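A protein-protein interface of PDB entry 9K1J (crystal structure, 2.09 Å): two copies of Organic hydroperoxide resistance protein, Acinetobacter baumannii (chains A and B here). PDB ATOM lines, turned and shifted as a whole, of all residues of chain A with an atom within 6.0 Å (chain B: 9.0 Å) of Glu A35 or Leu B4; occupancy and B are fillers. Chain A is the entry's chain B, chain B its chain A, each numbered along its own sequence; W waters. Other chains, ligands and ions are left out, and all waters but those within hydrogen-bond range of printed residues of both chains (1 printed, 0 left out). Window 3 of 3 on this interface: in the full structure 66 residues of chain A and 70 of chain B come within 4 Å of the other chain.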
ATOM      1  N   PRO A  33     -29.315   2.921  19.469  1.00  0.00           N
ATOM      2  CA  PRO A  33     -29.642   1.784  18.599  1.00  0.00           C
ATOM      3  C   PRO A  33     -29.673   0.496  19.421  1.00  0.00           C
ATOM      4  O   PRO A  33     -29.148   0.444  20.534  1.00  0.00           O
ATOM      5  CB  PRO A  33     -28.498   1.779  17.580  1.00  0.00           C
ATOM      6  CG  PRO A  33     -27.343   2.419  18.342  1.00  0.00           C
ATOM      7  CD  PRO A  33     -27.955   3.444  19.237  1.00  0.00           C
ATOM      8  N   LYS A  34     -30.306  -0.558  18.873  1.00  0.00           N
ATOM      9  CA  LYS A  34     -30.416  -1.811  19.641  1.00  0.00           C
ATOM     10  C   LYS A  34     -29.045  -2.367  20.020  1.00  0.00           C
ATOM     11  O   LYS A  34     -28.874  -2.908  21.121  1.00  0.00           O
ATOM     12  CB  LYS A  34     -31.237  -2.900  18.919  1.00  0.00           C
ATOM     13  CG  LYS A  34     -32.740  -2.613  18.829  1.00  0.00           C
ATOM     14  CD  LYS A  34     -33.533  -3.750  18.144  1.00  0.00           C
ATOM     15  CE  LYS A  34     -33.709  -4.970  19.094  1.00  0.00           C
ATOM     16  NZ  LYS A  34     -34.582  -4.624  20.280  1.00  0.00           N
ATOM     17  N   GLU A  35     -28.044  -2.203  19.149  1.00  0.00           N
ATOM     18  CA  GLU A  35     -26.719  -2.739  19.460  1.00  0.00           C
ATOM     19  C   GLU A  35     -26.140  -2.151  20.741  1.00  0.00           C
ATOM     20  O   GLU A  35     -25.273  -2.772  21.364  1.00  0.00           O
ATOM     21  CB  GLU A  35     -25.730  -2.500  18.308  1.00  0.00           C
ATOM     22  CG  GLU A  35     -26.061  -3.201  17.000  1.00  0.00           C
ATOM     23  CD  GLU A  35     -26.829  -2.328  16.038  1.00  0.00           C
ATOM     24  OE1 GLU A  35     -27.742  -1.592  16.473  1.00  0.00           O
ATOM     25  OE2 GLU A  35     -26.493  -2.362  14.835  1.00  0.00           O
ATOM     26  N   LEU A  36     -26.607  -0.976  21.155  1.00  0.00           N
ATOM     27  CA  LEU A  36     -26.194  -0.369  22.414  1.00  0.00           C
ATOM     28  C   LEU A  36     -27.317  -0.386  23.451  1.00  0.00           C
ATOM     29  O   LEU A  36     -27.344   0.454  24.351  1.00  0.00           O
ATOM     30  CB  LEU A  36     -25.697   1.061  22.184  1.00  0.00           C
ATOM     31  CG  LEU A  36     -24.727   1.318  21.020  1.00  0.00           C
ATOM     32  CD1 LEU A  36     -24.304   2.780  20.990  1.00  0.00           C
ATOM     33  CD2 LEU A  36     -23.506   0.399  21.075  1.00  0.00           C
ATOM     34  N   GLY A  37     -28.256  -1.322  23.325  1.00  0.00           N
ATOM     35  CA  GLY A  37     -29.270  -1.519  24.343  1.00  0.00           C
ATOM     36  C   GLY A  37     -30.479  -0.617  24.242  1.00  0.00           C
ATOM     37  O   GLY A  37     -31.124  -0.356  25.260  1.00  0.00           O
ATOM     38  N   GLY A  38     -30.810  -0.135  23.046  1.00  0.00           N
ATOM     39  CA  GLY A  38     -31.990   0.692  22.857  1.00  0.00           C
ATOM     40  C   GLY A  38     -32.971   0.104  21.863  1.00  0.00           C
ATOM     41  O   GLY A  38     -32.882  -1.083  21.543  1.00  0.00           O
ATOM     42  N   ILE A  86     -18.378   3.278  16.341  1.00  0.00           N
ATOM     43  CA  ILE A  86     -17.866   3.642  17.655  1.00  0.00           C
ATOM     44  C   ILE A  86     -17.217   2.390  18.245  1.00  0.00           C
ATOM     45  O   ILE A  86     -17.818   1.312  18.236  1.00  0.00           O
ATOM     46  CB  ILE A  86     -18.983   4.238  18.542  1.00  0.00           C
ATOM     47  CG1 ILE A  86     -18.462   4.624  19.936  1.00  0.00           C
ATOM     48  CG2 ILE A  86     -20.221   3.345  18.571  1.00  0.00           C
ATOM     49  CD1 ILE A  86     -19.252   5.787  20.589  1.00  0.00           C
ATOM     50  N   VAL A  87     -15.957   2.512  18.657  1.00  0.00           N
ATOM     51  CA  VAL A  87     -15.145   1.391  19.114  1.00  0.00           C
ATOM     52  C   VAL A  87     -14.668   1.682  20.531  1.00  0.00           C
ATOM     53  O   VAL A  87     -14.634   2.835  20.972  1.00  0.00           O
ATOM     54  CB  VAL A  87     -13.926   1.107  18.199  1.00  0.00           C
ATOM     55  CG1 VAL A  87     -14.358   0.751  16.798  1.00  0.00           C
ATOM     56  CG2 VAL A  87     -12.967   2.291  18.186  1.00  0.00           C
ATOM     57  N   ALA A  88     -14.311   0.624  21.252  1.00  0.00           N
ATOM     58  CA  ALA A  88     -13.686   0.791  22.560  1.00  0.00           C
ATOM     59  C   ALA A  88     -12.224   1.201  22.401  1.00  0.00           C
ATOM     60  O   ALA A  88     -11.467   0.516  21.706  1.00  0.00           O
ATOM     61  CB  ALA A  88     -13.789  -0.512  23.345  1.00  0.00           C
ATOM     62  N   PHE A  94     -14.157   5.375  24.392  1.00  0.00           N
ATOM     63  CA  PHE A  94     -14.741   5.144  23.077  1.00  0.00           C
ATOM     64  C   PHE A  94     -14.156   6.112  22.056  1.00  0.00           C
ATOM     65  O   PHE A  94     -13.875   7.273  22.373  1.00  0.00           O
ATOM     66  CB  PHE A  94     -16.263   5.275  23.136  1.00  0.00           C
ATOM     67  CG  PHE A  94     -16.902   4.308  24.084  1.00  0.00           C
ATOM     68  CD1 PHE A  94     -17.127   2.993  23.711  1.00  0.00           C
ATOM     69  CD2 PHE A  94     -17.226   4.704  25.371  1.00  0.00           C
ATOM     70  CE1 PHE A  94     -17.697   2.094  24.598  1.00  0.00           C
ATOM     71  CE2 PHE A  94     -17.797   3.816  26.261  1.00  0.00           C
ATOM     72  CZ  PHE A  94     -18.035   2.509  25.875  1.00  0.00           C
ATOM     73  N   SER B   2     -12.930  -3.548  19.290  1.00  0.00           N
ATOM     74  CA  SER B   2     -13.921  -3.966  18.294  1.00  0.00           C
ATOM     75  C   SER B   2     -15.080  -2.984  18.189  1.00  0.00           C
ATOM     76  O   SER B   2     -15.399  -2.280  19.149  1.00  0.00           O
ATOM     77  CB  SER B   2     -14.466  -5.358  18.614  1.00  0.00           C
ATOM     78  OG  SER B   2     -13.621  -6.362  18.093  1.00  0.00           O
ATOM     79  N   THR B   3     -15.724  -2.982  17.022  1.00  0.00           N
ATOM     80  CA  THR B   3     -16.752  -1.999  16.689  1.00  0.00           C
ATOM     81  C   THR B   3     -18.095  -2.339  17.340  1.00  0.00           C
ATOM     82  O   THR B   3     -18.706  -3.366  17.038  1.00  0.00           O
ATOM     83  CB  THR B   3     -16.857  -1.871  15.171  1.00  0.00           C
ATOM     84  OG1 THR B   3     -17.905  -0.945  14.835  1.00  0.00           O
ATOM     85  CG2 THR B   3     -17.026  -3.226  14.473  1.00  0.00           C
ATOM     86  N   LEU B   4     -18.565  -1.450  18.224  1.00  0.00           N
ATOM     87  CA  LEU B   4     -19.776  -1.707  19.001  1.00  0.00           C
ATOM     88  C   LEU B   4     -21.029  -1.390  18.199  1.00  0.00           C
ATOM     89  O   LEU B   4     -22.074  -2.031  18.375  1.00  0.00           O
ATOM     90  CB  LEU B   4     -19.748  -0.878  20.284  1.00  0.00           C
ATOM     91  CG  LEU B   4     -18.685  -1.303  21.298  1.00  0.00           C
ATOM     92  CD1 LEU B   4     -18.149  -0.096  22.017  1.00  0.00           C
ATOM     93  CD2 LEU B   4     -19.266  -2.290  22.299  1.00  0.00           C
ATOM     94  N   TYR B   5     -20.941  -0.394  17.322  1.00  0.00           N
ATOM     95  CA  TYR B   5     -22.072   0.043  16.521  1.00  0.00           C
ATOM     96  C   TYR B   5     -21.522   0.724  15.284  1.00  0.00           C
ATOM     97  O   TYR B   5     -20.577   1.506  15.367  1.00  0.00           O
ATOM     98  CB  TYR B   5     -22.986   1.001  17.289  1.00  0.00           C
ATOM     99  CG  TYR B   5     -24.054   1.656  16.434  1.00  0.00           C
ATOM    100  CD1 TYR B   5     -25.126   0.918  15.905  1.00  0.00           C
ATOM    101  CD2 TYR B   5     -23.987   3.024  16.138  1.00  0.00           C
ATOM    102  CE1 TYR B   5     -26.103   1.536  15.106  1.00  0.00           C
ATOM    103  CE2 TYR B   5     -24.946   3.642  15.362  1.00  0.00           C
ATOM    104  CZ  TYR B   5     -26.002   2.904  14.844  1.00  0.00           C
ATOM    105  OH  TYR B   5     -26.947   3.567  14.072  1.00  0.00           O
ATOM    106  N   SER B   6     -22.121   0.442  14.149  1.00  0.00           N
ATOM    107  CA  SER B   6     -21.669   1.040  12.910  1.00  0.00           C
ATOM    108  C   SER B   6     -22.895   1.468  12.125  1.00  0.00           C
ATOM    109  O   SER B   6     -23.930   0.800  12.179  1.00  0.00           O
ATOM    110  CB  SER B   6     -20.815   0.044  12.136  1.00  0.00           C
ATOM    111  OG  SER B   6     -20.307   0.611  10.960  1.00  0.00           O
ATOM    112  N   THR B   7     -22.799   2.594  11.417  1.00  0.00           N
ATOM    113  CA  THR B   7     -23.937   3.080  10.651  1.00  0.00           C
ATOM    114  C   THR B   7     -23.448   3.664   9.336  1.00  0.00           C
ATOM    115  O   THR B   7     -22.326   4.162   9.245  1.00  0.00           O
ATOM    116  CB  THR B   7     -24.763   4.133  11.447  1.00  0.00           C
ATOM    117  OG1 THR B   7     -25.946   4.498  10.719  1.00  0.00           O
ATOM    118  CG2 THR B   7     -23.944   5.405  11.756  1.00  0.00           C
ATOM    119  N   ASP B  23     -30.572   2.499   6.945  1.00  0.00           N
ATOM    120  CA  ASP B  23     -31.739   1.945   7.623  1.00  0.00           C
ATOM    121  C   ASP B  23     -32.973   2.851   7.543  1.00  0.00           C
ATOM    122  O   ASP B  23     -33.990   2.539   8.168  1.00  0.00           O
ATOM    123  CB  ASP B  23     -31.370   1.618   9.084  1.00  0.00           C
ATOM    124  CG  ASP B  23     -31.045   2.862   9.924  1.00  0.00           C
ATOM    125  OD1 ASP B  23     -31.096   4.011   9.406  1.00  0.00           O
ATOM    126  OD2 ASP B  23     -30.692   2.674  11.117  1.00  0.00           O
ATOM    127  N   ILE B  25     -33.798   5.639   8.834  1.00  0.00           N
ATOM    128  CA  ILE B  25     -34.240   6.397  10.002  1.00  0.00           C
ATOM    129  C   ILE B  25     -33.946   7.886   9.851  1.00  0.00           C
ATOM    130  O   ILE B  25     -34.723   8.734  10.305  1.00  0.00           O
ATOM    131  CB  ILE B  25     -33.614   5.803  11.278  1.00  0.00           C
ATOM    132  CG1 ILE B  25     -34.305   4.479  11.625  1.00  0.00           C
ATOM    133  CG2 ILE B  25     -33.670   6.785  12.429  1.00  0.00           C
ATOM    134  CD1 ILE B  25     -33.406   3.456  12.223  1.00  0.00           C
HETATM  135  O   HOH W   1     -23.639  -2.030  14.139  1.00  0.00           O
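N of Ile A86 is in hydrogen-bond range of O of Tyr B5 (3.0 Å). The backbone carbonyl oxygen (O) of Ile A86 sits at hydrogen-bond distance from the backbone NH (N) of Leu B4.
N of Gly A38 lies within hydrogen-bond range of O of Pro A33 (3.1 Å).
Among the printed residues, merely in contact across the chains: Phe A94 with Leu B4, Pro A33 with Tyr B5, Val A87 with Thr B3, Glu A35 with Tyr B5, Val A87 with Ser B2, Glu A35 with Leu B4, Ala A88 with Ser B2, Ile A86 with Thr B3, Leu A36 with Tyr B5, Leu A36 with Leu B4 and Ala A88 with Leu B4.
Printed residues of chain B within 4 Å of Pro A33: Tyr B5 (3.5 Å). Of chain B, only Leu B4 (3.7 Å) and Tyr B5 (3.7 Å) come within 4 Å of Glu A35. Of the printed residues of chain B, Leu A36 touches Leu B4 (3.9 Å) and Tyr B5 (3.9 Å). Printed residues of chain B within 4 Å of Val A87: Ser B2 (3.7 Å) and Thr B3 (3.6 Å). Printed residues of chain A within 4 Å of Ser B2: Val A87 (3.7 Å) and Ala A88 (3.7 Å). Of chain A, only Glu A35 (3.7 Å), Leu A36 (3.9 Å), Ile A86 (2.9 Å), Ala A88 (3.98 Å) and Phe A94 (3.4 Å) come within 4 Å of Leu B4. Printed residues of chain A within 4 Å of Tyr B5: Pro A33, Glu A35, Leu A36 and Ile A86. Ser B6 touches none of the printed residues of chain A.
Of the 8 printed residues of chain B, 4 touch a printed residue of chain A. Printed residues of chain B that touch a printed residue of chain A: Ser B2, Thr B3, Leu B4 and Tyr B5. Hydrophobic or aromatic side chains of chain A that line the printed part of chain B: Pro A33, Leu A36, Ile A86, Val A87 and Phe A94. Among the printed residues, 13 pairs touch across the chains.
No position is printed for both chains. Of the 13 pairs that touch across the chains among the printed residues, none has its exchanged pair printed and touching as well.
Water W1 lies within hydrogen-bond range of the backbone NH (N) of Ser B6 (2.9 Å) and the side-chain carboxylate (OE2) of Glu A35 (3.0 Å).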
